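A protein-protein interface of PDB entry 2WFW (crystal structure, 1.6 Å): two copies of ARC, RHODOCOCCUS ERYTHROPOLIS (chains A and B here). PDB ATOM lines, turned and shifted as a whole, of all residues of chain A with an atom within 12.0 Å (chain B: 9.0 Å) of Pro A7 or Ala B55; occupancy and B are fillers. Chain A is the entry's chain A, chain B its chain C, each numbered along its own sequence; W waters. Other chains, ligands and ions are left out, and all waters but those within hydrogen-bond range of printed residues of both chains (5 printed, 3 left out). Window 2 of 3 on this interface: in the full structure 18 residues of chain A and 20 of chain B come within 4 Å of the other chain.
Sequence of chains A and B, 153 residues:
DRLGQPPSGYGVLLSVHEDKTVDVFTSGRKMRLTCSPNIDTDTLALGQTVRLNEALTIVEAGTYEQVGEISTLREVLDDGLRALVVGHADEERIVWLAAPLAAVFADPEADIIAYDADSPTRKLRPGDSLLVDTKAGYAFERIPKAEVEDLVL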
ATOM      1  N   PRO A   7       8.266  -2.880  11.020  1.00  0.00           N
ATOM      2  CA  PRO A   7       9.479  -2.225  11.541  1.00  0.00           C
ATOM      3  C   PRO A   7      10.608  -2.286  10.522  1.00  0.00           C
ATOM      4  O   PRO A   7      10.735  -3.295   9.796  1.00  0.00           O
ATOM      5  CB  PRO A   7       9.828  -3.074  12.762  1.00  0.00           C
ATOM      6  CG  PRO A   7       8.469  -3.630  13.234  1.00  0.00           C
ATOM      7  CD  PRO A   7       7.489  -3.511  12.103  1.00  0.00           C
ATOM      8  N   SER A   8      11.415  -1.232  10.451  1.00  0.00           N
ATOM      9  CA  SER A   8      12.548  -1.192   9.510  1.00  0.00           C
ATOM     10  C   SER A   8      13.874  -1.022  10.246  1.00  0.00           C
ATOM     11  O   SER A   8      13.912  -0.433  11.335  1.00  0.00           O
ATOM     12  CB  SER A   8      12.444   0.014   8.583  1.00  0.00           C
ATOM     13  OG  SER A   8      11.205   0.155   7.973  1.00  0.00           O
ATOM     14  N   GLY A   9      14.942  -1.548   9.653  1.00  0.00           N
ATOM     15  CA  GLY A   9      16.310  -1.280  10.131  1.00  0.00           C
ATOM     16  C   GLY A   9      17.001  -0.348   9.136  1.00  0.00           C
ATOM     17  O   GLY A   9      16.377   0.154   8.188  1.00  0.00           O
ATOM     18  N   TYR A  10      18.295  -0.135   9.360  1.00  0.00           N
ATOM     19  CA  TYR A  10      19.049   0.786   8.556  1.00  0.00           C
ATOM     20  C   TYR A  10      20.436   0.245   8.311  1.00  0.00           C
ATOM     21  O   TYR A  10      20.943  -0.630   9.029  1.00  0.00           O
ATOM     22  CB  TYR A  10      19.206   2.137   9.275  1.00  0.00           C
ATOM     23  CG  TYR A  10      17.930   2.950   9.340  1.00  0.00           C
ATOM     24  CD1 TYR A  10      17.543   3.720   8.260  1.00  0.00           C
ATOM     25  CD2 TYR A  10      17.133   2.979  10.502  1.00  0.00           C
ATOM     26  CE1 TYR A  10      16.383   4.486   8.285  1.00  0.00           C
ATOM     27  CE2 TYR A  10      15.955   3.767  10.561  1.00  0.00           C
ATOM     28  CZ  TYR A  10      15.587   4.532   9.454  1.00  0.00           C
ATOM     29  OH  TYR A  10      14.456   5.311   9.492  1.00  0.00           O
ATOM     30  N   GLY A  11      21.053   0.774   7.265  1.00  0.00           N
ATOM     31  CA  GLY A  11      22.480   0.497   7.005  1.00  0.00           C
ATOM     32  C   GLY A  11      23.097   1.632   6.218  1.00  0.00           C
ATOM     33  O   GLY A  11      22.426   2.594   5.851  1.00  0.00           O
ATOM     34  N   THR A  26      25.500  -3.145   7.588  1.00  0.00           N
ATOM     35  CA  THR A  26      24.339  -3.187   8.490  1.00  0.00           C
ATOM     36  C   THR A  26      24.508  -4.359   9.443  1.00  0.00           C
ATOM     37  O   THR A  26      25.121  -5.336   9.092  1.00  0.00           O
ATOM     38  CB  THR A  26      22.997  -3.242   7.727  1.00  0.00           C
ATOM     39  OG1 THR A  26      21.892  -3.137   8.648  1.00  0.00           O
ATOM     40  CG2 THR A  26      22.865  -4.564   6.976  1.00  0.00           C
ATOM     41  N   SER A  27      23.951  -4.226  10.649  1.00  0.00           N
ATOM     42  CA  SER A  27      24.182  -5.221  11.699  1.00  0.00           C
ATOM     43  C   SER A  27      25.672  -5.573  11.834  1.00  0.00           C
ATOM     44  O   SER A  27      26.031  -6.761  11.991  1.00  0.00           O
ATOM     45  CB  SER A  27      23.371  -6.491  11.436  1.00  0.00           C
ATOM     46  OG  SER A  27      21.998  -6.220  11.417  1.00  0.00           O
ATOM     47  N   VAL A  50      20.523   3.861   4.174  1.00  0.00           N
ATOM     48  CA  VAL A  50      19.398   3.182   3.513  1.00  0.00           C
ATOM     49  C   VAL A  50      18.544   2.475   4.547  1.00  0.00           C
ATOM     50  O   VAL A  50      19.062   1.981   5.568  1.00  0.00           O
ATOM     51  CB  VAL A  50      19.838   2.198   2.391  1.00  0.00           C
ATOM     52  CG1 VAL A  50      20.465   2.982   1.239  1.00  0.00           C
ATOM     53  CG2 VAL A  50      20.808   1.135   2.922  1.00  0.00           C
ATOM     54  N   ARG A  51      17.230   2.482   4.287  1.00  0.00           N
ATOM     55  CA  ARG A  51      16.240   1.823   5.158  1.00  0.00           C
ATOM     56  C   ARG A  51      15.936   0.424   4.633  1.00  0.00           C
ATOM     57  O   ARG A  51      15.750   0.254   3.408  1.00  0.00           O
ATOM     58  CB  ARG A  51      14.961   2.648   5.226  1.00  0.00           C
ATOM     59  CG  ARG A  51      14.105   2.156   6.367  1.00  0.00           C
ATOM     60  CD  ARG A  51      13.055   3.198   6.771  1.00  0.00           C
ATOM     61  NE  ARG A  51      12.227   3.667   5.652  1.00  0.00           N
ATOM     62  CZ  ARG A  51      11.111   3.071   5.242  1.00  0.00           C
ATOM     63  NH1 ARG A  51      10.646   1.983   5.861  1.00  0.00           N
ATOM     64  NH2 ARG A  51      10.429   3.578   4.208  1.00  0.00           N
ATOM     65  N   LEU A  52      15.867  -0.551   5.538  1.00  0.00           N
ATOM     66  CA  LEU A  52      15.746  -1.971   5.147  1.00  0.00           C
ATOM     67  C   LEU A  52      14.463  -2.532   5.776  1.00  0.00           C
ATOM     68  O   LEU A  52      14.181  -2.307   6.969  1.00  0.00           O
ATOM     69  CB  LEU A  52      16.939  -2.769   5.709  1.00  0.00           C
ATOM     70  CG  LEU A  52      18.311  -2.187   5.398  1.00  0.00           C
ATOM     71  CD1 LEU A  52      19.348  -3.012   6.169  1.00  0.00           C
ATOM     72  CD2 LEU A  52      18.536  -2.233   3.900  1.00  0.00           C
ATOM     73  N   ASN A  53      13.687  -3.286   5.011  1.00  0.00           N
ATOM     74  CA  ASN A  53      12.557  -3.994   5.643  1.00  0.00           C
ATOM     75  C   ASN A  53      13.023  -5.297   6.336  1.00  0.00           C
ATOM     76  O   ASN A  53      14.246  -5.567   6.389  1.00  0.00           O
ATOM     77  CB  ASN A  53      11.426  -4.226   4.623  1.00  0.00           C
ATOM     78  CG  ASN A  53      11.792  -5.231   3.525  1.00  0.00           C
ATOM     79  OD1 ASN A  53      12.817  -5.927   3.596  1.00  0.00           O
ATOM     80  ND2 ASN A  53      10.934  -5.306   2.500  1.00  0.00           N
ATOM     81  N   GLU A  54      12.074  -6.059   6.910  1.00  0.00           N
ATOM     82  CA  GLU A  54      12.419  -7.272   7.658  1.00  0.00           C
ATOM     83  C   GLU A  54      13.226  -8.265   6.827  1.00  0.00           C
ATOM     84  O   GLU A  54      14.089  -8.978   7.378  1.00  0.00           O
ATOM     85  CB  GLU A  54      11.169  -8.006   8.155  1.00  0.00           C
ATOM     86  CG  GLU A  54       9.881  -7.191   8.148  1.00  0.00           C
ATOM     87  CD  GLU A  54       9.795  -6.377   9.398  1.00  0.00           C
ATOM     88  OE1 GLU A  54      10.861  -6.292  10.043  1.00  0.00           O
ATOM     89  OE2 GLU A  54       8.698  -5.861   9.761  1.00  0.00           O
ATOM     90  N   ALA A  55      12.954  -8.285   5.522  1.00  0.00           N
ATOM     91  CA  ALA A  55      13.628  -9.182   4.578  1.00  0.00           C
ATOM     92  C   ALA A  55      14.985  -8.651   4.123  1.00  0.00           C
ATOM     93  O   ALA A  55      15.651  -9.309   3.356  1.00  0.00           O
ATOM     94  CB  ALA A  55      12.746  -9.454   3.389  1.00  0.00           C
ATOM     95  N   LEU A  56      15.370  -7.469   4.608  1.00  0.00           N
ATOM     96  CA  LEU A  56      16.657  -6.802   4.268  1.00  0.00           C
ATOM     97  C   LEU A  56      16.673  -6.260   2.842  1.00  0.00           C
ATOM     98  O   LEU A  56      17.731  -6.066   2.274  1.00  0.00           O
ATOM     99  CB  LEU A  56      17.906  -7.679   4.554  1.00  0.00           C
ATOM    100  CG  LEU A  56      17.983  -8.258   5.964  1.00  0.00           C
ATOM    101  CD1 LEU A  56      19.327  -9.022   6.172  1.00  0.00           C
ATOM    102  CD2 LEU A  56      17.830  -7.168   7.027  1.00  0.00           C
ATOM    103  N   THR A  57      15.481  -6.003   2.295  1.00  0.00           N
ATOM    104  CA  THR A  57      15.372  -5.275   1.014  1.00  0.00           C
ATOM    105  C   THR A  57      15.508  -3.773   1.288  1.00  0.00           C
ATOM    106  O   THR A  57      14.923  -3.266   2.253  1.00  0.00           O
ATOM    107  CB  THR A  57      13.999  -5.544   0.392  1.00  0.00           C
ATOM    108  OG1 THR A  57      13.890  -6.950   0.085  1.00  0.00           O
ATOM    109  CG2 THR A  57      13.765  -4.703  -0.881  1.00  0.00           C
ATOM    110  N   ILE A  58      16.289  -3.074   0.466  1.00  0.00           N
ATOM    111  CA  ILE A  58      16.344  -1.599   0.597  1.00  0.00           C
ATOM    112  C   ILE A  58      15.020  -0.996   0.124  1.00  0.00           C
ATOM    113  O   ILE A  58      14.611  -1.161  -1.041  1.00  0.00           O
ATOM    114  CB  ILE A  58      17.508  -0.945  -0.223  1.00  0.00           C
ATOM    115  CG1 ILE A  58      18.885  -1.266   0.387  1.00  0.00           C
ATOM    116  CG2 ILE A  58      17.330   0.578  -0.311  1.00  0.00           C
ATOM    117  CD1 ILE A  58      19.270  -2.727   0.373  1.00  0.00           C
ATOM    118  N   VAL A  59      14.371  -0.291   1.033  1.00  0.00           N
ATOM    119  CA  VAL A  59      13.060   0.300   0.714  1.00  0.00           C
ATOM    120  C   VAL A  59      13.057   1.839   0.589  1.00  0.00           C
ATOM    121  O   VAL A  59      12.077   2.434   0.108  1.00  0.00           O
ATOM    122  CB  VAL A  59      11.948  -0.198   1.686  1.00  0.00           C
ATOM    123  CG1 VAL A  59      11.726  -1.720   1.495  1.00  0.00           C
ATOM    124  CG2 VAL A  59      12.276   0.186   3.165  1.00  0.00           C
ATOM    125  N   GLU A  60      14.141   2.479   1.027  1.00  0.00           N
ATOM    126  CA  GLU A  60      14.228   3.942   0.996  1.00  0.00           C
ATOM    127  C   GLU A  60      15.679   4.365   1.118  1.00  0.00           C
ATOM    128  O   GLU A  60      16.462   3.697   1.801  1.00  0.00           O
ATOM    129  CB  GLU A  60      13.406   4.580   2.130  1.00  0.00           C
ATOM    130  CG  GLU A  60      13.221   6.114   1.951  1.00  0.00           C
ATOM    131  CD  GLU A  60      12.310   6.746   3.013  1.00  0.00           C
ATOM    132  OE1 GLU A  60      11.938   6.056   3.988  1.00  0.00           O
ATOM    133  OE2 GLU A  60      11.974   7.946   2.863  1.00  0.00           O
ATOM    134  N   PRO B   7       6.225  -9.238  27.991  1.00  0.00           N
ATOM    135  CA  PRO B   7       7.220  -8.220  28.294  1.00  0.00           C
ATOM    136  C   PRO B   7       7.223  -7.067  27.292  1.00  0.00           C
ATOM    137  O   PRO B   7       6.838  -7.246  26.122  1.00  0.00           O
ATOM    138  CB  PRO B   7       8.537  -8.987  28.157  1.00  0.00           C
ATOM    139  CG  PRO B   7       8.198 -10.384  28.572  1.00  0.00           C
ATOM    140  CD  PRO B   7       6.762 -10.606  28.148  1.00  0.00           C
ATOM    141  N   SER B   8       7.663  -5.887  27.736  1.00  0.00           N
ATOM    142  CA  SER B   8       7.853  -4.756  26.823  1.00  0.00           C
ATOM    143  C   SER B   8       9.353  -4.441  26.739  1.00  0.00           C
ATOM    144  O   SER B   8      10.083  -4.558  27.731  1.00  0.00           O
ATOM    145  CB  SER B   8       7.125  -3.476  27.320  1.00  0.00           C
ATOM    146  OG  SER B   8       5.727  -3.655  27.529  1.00  0.00           O
ATOM    147  N   GLY B   9       9.804  -4.034  25.560  1.00  0.00           N
ATOM    148  CA  GLY B   9      11.108  -3.395  25.461  1.00  0.00           C
ATOM    149  C   GLY B   9      11.017  -1.875  25.539  1.00  0.00           C
ATOM    150  O   GLY B   9       9.939  -1.290  25.698  1.00  0.00           O
ATOM    151  N   THR B  21       5.728   7.782  11.544  1.00  0.00           N
ATOM    152  CA  THR B  21       6.639   6.769  12.071  1.00  0.00           C
ATOM    153  C   THR B  21       7.735   7.506  12.844  1.00  0.00           C
ATOM    154  O   THR B  21       7.871   8.723  12.721  1.00  0.00           O
ATOM    155  CB  THR B  21       7.272   5.878  10.973  1.00  0.00           C
ATOM    156  OG1 THR B  21       8.017   6.699  10.072  1.00  0.00           O
ATOM    157  CG2 THR B  21       6.188   5.091  10.175  1.00  0.00           C
ATOM    158  N   VAL B  22       8.548   6.746  13.585  1.00  0.00           N
ATOM    159  CA  VAL B  22       9.548   7.337  14.461  1.00  0.00           C
ATOM    160  C   VAL B  22      10.834   6.515  14.357  1.00  0.00           C
ATOM    161  O   VAL B  22      10.770   5.279  14.301  1.00  0.00           O
ATOM    162  CB  VAL B  22       9.044   7.311  15.934  1.00  0.00           C
ATOM    163  CG1 VAL B  22       7.848   8.280  16.104  1.00  0.00           C
ATOM    164  CG2 VAL B  22       8.674   5.906  16.357  1.00  0.00           C
ATOM    165  N   THR B  26      16.939   1.048  19.875  1.00  0.00           N
ATOM    166  CA  THR B  26      16.426   0.000  20.745  1.00  0.00           C
ATOM    167  C   THR B  26      17.195  -1.296  20.480  1.00  0.00           C
ATOM    168  O   THR B  26      17.556  -1.588  19.335  1.00  0.00           O
ATOM    169  CB  THR B  26      14.900  -0.233  20.533  1.00  0.00           C
ATOM    170  OG1 THR B  26      14.449  -1.214  21.465  1.00  0.00           O
ATOM    171  CG2 THR B  26      14.564  -0.688  19.086  1.00  0.00           C
ATOM    172  N   ARG B  29      20.337  -0.907  18.207  1.00  0.00           N
ATOM    173  CA  ARG B  29      20.351  -0.404  16.830  1.00  0.00           C
ATOM    174  C   ARG B  29      19.202   0.536  16.534  1.00  0.00           C
ATOM    175  O   ARG B  29      18.199   0.548  17.249  1.00  0.00           O
ATOM    176  CB  ARG B  29      20.378  -1.532  15.813  1.00  0.00           C
ATOM    177  CG  ARG B  29      19.094  -2.239  15.642  1.00  0.00           C
ATOM    178  CD  ARG B  29      19.362  -3.410  14.700  1.00  0.00           C
ATOM    179  NE  ARG B  29      18.296  -4.405  14.666  1.00  0.00           N
ATOM    180  CZ  ARG B  29      17.459  -4.571  13.642  1.00  0.00           C
ATOM    181  NH1 ARG B  29      17.540  -3.774  12.570  1.00  0.00           N
ATOM    182  NH2 ARG B  29      16.520  -5.510  13.701  1.00  0.00           N
ATOM    183  N   LYS B  30      19.395   1.296  15.470  1.00  0.00           N
ATOM    184  CA  LYS B  30      18.389   2.260  14.982  1.00  0.00           C
ATOM    185  C   LYS B  30      17.309   1.525  14.181  1.00  0.00           C
ATOM    186  O   LYS B  30      17.614   0.724  13.269  1.00  0.00           O
ATOM    187  CB  LYS B  30      19.083   3.283  14.080  1.00  0.00           C
ATOM    188  CG  LYS B  30      18.276   4.544  13.826  1.00  0.00           C
ATOM    189  CD  LYS B  30      19.023   5.607  12.975  1.00  0.00           C
ATOM    190  CE  LYS B  30      18.217   5.805  11.644  1.00  0.00           C
ATOM    191  NZ  LYS B  30      18.645   6.735  10.504  1.00  0.00           N
ATOM    192  N   MET B  31      16.050   1.783  14.529  1.00  0.00           N
ATOM    193  CA  MET B  31      14.903   1.215  13.821  1.00  0.00           C
ATOM    194  C   MET B  31      13.893   2.258  13.481  1.00  0.00           C
ATOM    195  O   MET B  31      13.787   3.244  14.196  1.00  0.00           O
ATOM    196  CB  MET B  31      14.208   0.140  14.659  1.00  0.00           C
ATOM    197  CG  MET B  31      15.111  -0.912  15.193  1.00  0.00           C
ATOM    198  SD  MET B  31      14.216  -2.369  15.707  1.00  0.00           S
ATOM    199  CE  MET B  31      13.820  -3.071  14.087  1.00  0.00           C
ATOM    200  N   ARG B  32      13.106   2.013  12.439  1.00  0.00           N
ATOM    201  CA  ARG B  32      11.929   2.870  12.151  1.00  0.00           C
ATOM    202  C   ARG B  32      10.685   2.118  12.551  1.00  0.00           C
ATOM    203  O   ARG B  32      10.444   1.013  12.061  1.00  0.00           O
ATOM    204  CB  ARG B  32      11.846   3.208  10.658  1.00  0.00           C
ATOM    205  CG  ARG B  32      10.705   4.246  10.432  1.00  0.00           C
ATOM    206  CD  ARG B  32      10.610   4.681   8.976  1.00  0.00           C
ATOM    207  NE  ARG B  32      11.745   5.521   8.649  1.00  0.00           N
ATOM    208  CZ  ARG B  32      11.747   6.497   7.720  1.00  0.00           C
ATOM    209  NH1 ARG B  32      10.651   6.805   7.039  1.00  0.00           N
ATOM    210  NH2 ARG B  32      12.862   7.193   7.513  1.00  0.00           N
ATOM    211  N   LEU B  33       9.972   2.667  13.531  1.00  0.00           N
ATOM    212  CA  LEU B  33       8.805   1.985  14.118  1.00  0.00           C
ATOM    213  C   LEU B  33       7.510   2.794  13.991  1.00  0.00           C
ATOM    214  O   LEU B  33       7.511   4.030  13.785  1.00  0.00           O
ATOM    215  CB  LEU B  33       9.067   1.674  15.600  1.00  0.00           C
ATOM    216  CG  LEU B  33      10.373   0.942  15.887  1.00  0.00           C
ATOM    217  CD1 LEU B  33      10.541   0.843  17.408  1.00  0.00           C
ATOM    218  CD2 LEU B  33      10.357  -0.413  15.187  1.00  0.00           C
ATOM    219  N   THR B  34       6.385   2.096  14.166  1.00  0.00           N
ATOM    220  CA  THR B  34       5.050   2.701  14.133  1.00  0.00           C
ATOM    221  C   THR B  34       4.504   2.921  15.558  1.00  0.00           C
ATOM    222  O   THR B  34       4.803   2.114  16.441  1.00  0.00           O
ATOM    223  CB  THR B  34       4.099   1.773  13.383  1.00  0.00           C
ATOM    224  OG1 THR B  34       4.061   0.507  14.048  1.00  0.00           O
ATOM    225  CG2 THR B  34       4.563   1.581  11.974  1.00  0.00           C
ATOM    226  N   LEU B  52       7.947  -0.291  23.949  1.00  0.00           N
ATOM    227  CA  LEU B  52       7.580  -1.064  22.750  1.00  0.00           C
ATOM    228  C   LEU B  52       6.880  -2.347  23.150  1.00  0.00           C
ATOM    229  O   LEU B  52       7.301  -3.008  24.108  1.00  0.00           O
ATOM    230  CB  LEU B  52       8.853  -1.451  21.968  1.00  0.00           C
ATOM    231  CG  LEU B  52       9.808  -0.287  21.754  1.00  0.00           C
ATOM    232  CD1 LEU B  52      11.051  -0.796  21.035  1.00  0.00           C
ATOM    233  CD2 LEU B  52       9.091   0.811  20.948  1.00  0.00           C
ATOM    234  N   ASN B  53       5.825  -2.735  22.421  1.00  0.00           N
ATOM    235  CA  ASN B  53       5.325  -4.096  22.586  1.00  0.00           C
ATOM    236  C   ASN B  53       6.193  -5.115  21.838  1.00  0.00           C
ATOM    237  O   ASN B  53       7.222  -4.755  21.238  1.00  0.00           O
ATOM    238  CB  ASN B  53       3.828  -4.198  22.247  1.00  0.00           C
ATOM    239  CG  ASN B  53       3.522  -4.026  20.784  1.00  0.00           C
ATOM    240  OD1 ASN B  53       4.423  -4.050  19.914  1.00  0.00           O
ATOM    241  ND2 ASN B  53       2.217  -3.856  20.484  1.00  0.00           N
ATOM    242  N   GLU B  54       5.807  -6.391  21.907  1.00  0.00           N
ATOM    243  CA  GLU B  54       6.653  -7.426  21.329  1.00  0.00           C
ATOM    244  C   GLU B  54       6.776  -7.278  19.805  1.00  0.00           C
ATOM    245  O   GLU B  54       7.815  -7.618  19.240  1.00  0.00           O
ATOM    246  CB  GLU B  54       6.141  -8.811  21.711  1.00  0.00           C
ATOM    247  CG  GLU B  54       7.220  -9.752  22.249  1.00  0.00           C
ATOM    248  CD  GLU B  54       7.419 -10.994  21.371  1.00  0.00           C
ATOM    249  OE1 GLU B  54       6.403 -11.665  21.029  1.00  0.00           O
ATOM    250  OE2 GLU B  54       8.596 -11.315  21.048  1.00  0.00           O
ATOM    251  N   ALA B  55       5.732  -6.703  19.169  1.00  0.00           N
ATOM    252  CA  ALA B  55       5.712  -6.418  17.720  1.00  0.00           C
ATOM    253  C   ALA B  55       6.499  -5.140  17.342  1.00  0.00           C
ATOM    254  O   ALA B  55       6.574  -4.760  16.143  1.00  0.00           O
ATOM    255  CB  ALA B  55       4.267  -6.300  17.254  1.00  0.00           C
ATOM    256  N   LEU B  56       7.067  -4.492  18.357  1.00  0.00           N
ATOM    257  CA  LEU B  56       7.859  -3.251  18.226  1.00  0.00           C
ATOM    258  C   LEU B  56       7.047  -1.994  17.885  1.00  0.00           C
ATOM    259  O   LEU B  56       7.593  -0.998  17.414  1.00  0.00           O
ATOM    260  CB  LEU B  56       9.044  -3.415  17.247  1.00  0.00           C
ATOM    261  CG  LEU B  56       9.921  -4.652  17.497  1.00  0.00           C
ATOM    262  CD1 LEU B  56      11.154  -4.566  16.574  1.00  0.00           C
ATOM    263  CD2 LEU B  56      10.389  -4.716  18.952  1.00  0.00           C
ATOM    264  N   THR B  57       5.748  -2.040  18.175  1.00  0.00           N
ATOM    265  CA  THR B  57       4.929  -0.843  18.131  1.00  0.00           C
ATOM    266  C   THR B  57       5.201  -0.001  19.369  1.00  0.00           C
ATOM    267  O   THR B  57       5.315  -0.539  20.462  1.00  0.00           O
ATOM    268  CB  THR B  57       3.430  -1.245  18.115  1.00  0.00           C
ATOM    269  OG1 THR B  57       3.187  -2.077  16.959  1.00  0.00           O
ATOM    270  CG2 THR B  57       2.553   0.012  18.066  1.00  0.00           C
ATOM    271  N   ILE B  58       5.296   1.317  19.195  1.00  0.00           N
ATOM    272  CA  ILE B  58       5.462   2.213  20.336  1.00  0.00           C
ATOM    273  C   ILE B  58       4.103   2.325  21.029  1.00  0.00           C
ATOM    274  O   ILE B  58       3.082   2.781  20.415  1.00  0.00           O
ATOM    275  CB  ILE B  58       5.913   3.658  19.939  1.00  0.00           C
ATOM    276  CG1 ILE B  58       7.350   3.733  19.451  1.00  0.00           C
ATOM    277  CG2 ILE B  58       5.782   4.590  21.138  1.00  0.00           C
ATOM    278  CD1 ILE B  58       7.649   2.907  18.320  1.00  0.00           C
ATOM    279  N   VAL B  59       4.084   1.941  22.309  1.00  0.00           N
ATOM    280  CA  VAL B  59       2.814   1.913  23.077  1.00  0.00           C
ATOM    281  C   VAL B  59       2.698   2.959  24.169  1.00  0.00           C
ATOM    282  O   VAL B  59       1.590   3.169  24.712  1.00  0.00           O
ATOM    283  CB  VAL B  59       2.442   0.484  23.630  1.00  0.00           C
ATOM    284  CG1 VAL B  59       2.141  -0.475  22.467  1.00  0.00           C
ATOM    285  CG2 VAL B  59       3.527  -0.090  24.577  1.00  0.00           C
HETATM  286  O   HOH W   1      12.463   9.351   5.646  1.00  0.00           O
HETATM  287  O   HOH W   2      14.798   6.273   4.936  1.00  0.00           O
HETATM  288  O   HOH W   3      15.465   8.326   9.103  1.00  0.00           O
HETATM  289  O   HOH W   4      19.175  -1.054  12.083  1.00  0.00           O
HETATM  290  O   HOH W   5      10.060   8.495   4.778  1.00  0.00           O
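Pro A7 touches Ala B55, but with the chains exchanged Ala A55 does not touch Pro B7 (21.5 Å).
Positions printed for both chains: 7, 8, 9, 26, 52, 53, 54, 55, 56, 57, 58 and 59.
Of the 12 pairs that touch across the chains among the printed residues, none has its exchanged pair printed and touching as well.
Among the printed residues, pairs that only touch across the chains: Ser A8 with Met B31, Tyr A10 with Lys B30, Arg A51 with Arg B32, Pro A7 with Arg B32, Pro A7 with Leu B33, Pro A7 with Ala B55, Gly A9 with Arg B29, Tyr A10 with Met B31 and Gly A9 with Lys B30.
Hydrophobic or aromatic side chains of chain A that line the printed part of chain B: Pro A7 and Tyr A10.
Of the 20 printed residues of chain B, 6 touch a printed residue of chain A.
Hydrophobic or aromatic side chains of chain B within 4 Å of the printed part of chain A: Met B31 and Leu B33.
Among the printed residues, Asp or Glu carboxylates within 4 Å of a Lys or Arg side-chain nitrogen of the other chain: Glu A60 with Arg B32.
The side-chain hydroxyl (OG) of Ser A8 sits at hydrogen-bond distance from the guanidinium group (NH1) of Arg A51 (2.8 Å).
The backbone carbonyl oxygen of Gly A9 is in hydrogen-bond range of the backbone NH of Leu A52 (2.8 Å).
O of Tyr A10 is in hydrogen-bond range of OG1 of Thr A26 (2.7 Å).
The backbone carbonyl oxygen (O) of Arg A51 is in hydrogen-bond range of the backbone NH (N) of Val A59, at 2.8 Å.
The guanidinium group of Arg A51 is in salt-bridge range of the side-chain carboxylate of Glu A60, at 2.9 Å.
The side-chain amide oxygen of Asn B53 lies within hydrogen-bond range of the backbone NH of Ala B55, at 3.1 Å.
Water W4 lies within hydrogen-bond range of O of Lys B30 (2.6 Å), N of Tyr A10 (3.0 Å) and NH1 of Arg B29 (3.2 Å).
Water W5 lies within hydrogen-bond range of OE2 of Glu A60 (2.8 Å) and NH1 of Arg B32 (2.9 Å).
Water W1 lies within hydrogen-bond range of the guanidinium group (NH2) of Arg B32 and the side-chain carboxylate (OE2) of Glu A60.
Water W2 lies within hydrogen-bond range of the side-chain carboxylate of Glu A60 and the guanidinium group of Arg B32.
Water W3 bridges OH of Tyr A10 (3.2 Å) and NH2 of Arg B32 (3.3 Å).
O of Ser A8 is in hydrogen-bond range of N of Arg B32 (2.8 Å).
NE of Arg B32 sits at hydrogen-bond distance from OH of Tyr A10.
The side-chain carboxylate (OE1) of Glu A60 is in salt-bridge range of the guanidinium group (NH1) of Arg B32 (3.4 Å).
Pro A7 touches just these residues of chain B: Arg B32, Leu B33 and Ala B55.
Ser A27 touches none of the printed residues of chain B.
Of the printed residues of chain B, Arg A51 touches Arg B32.
Val A59 touches none of the printed residues of chain B.
Of the printed residues of chain A, Arg B29 touches Gly A9 (3.7 Å).
Of the printed residues of chain A, Lys B30 touches Gly A9 and Tyr A10.
Of chain A, only Ser A8 and Tyr A10 come within 4 Å of Met B31.
Leu B33 touches one residue of chain A.
No residue of chain A comes within 4 Å of Thr B34.
No residue of chain A comes within 4 Å of Asn B53.
Of chain A, only Pro A7 comes within 4 Å of Ala B55.
No residue of chain A comes within 4 Å of Leu B56.
The nearest residue of chain B that does not touch Pro A7 is Leu B56 (4.1 Å).
The nearest residue of chain A that does not touch Ala B55 is Glu A54 (6.8 Å).
The nearest printed residue of chain A that does not touch Arg B29 is Tyr A10 (4.9 Å).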
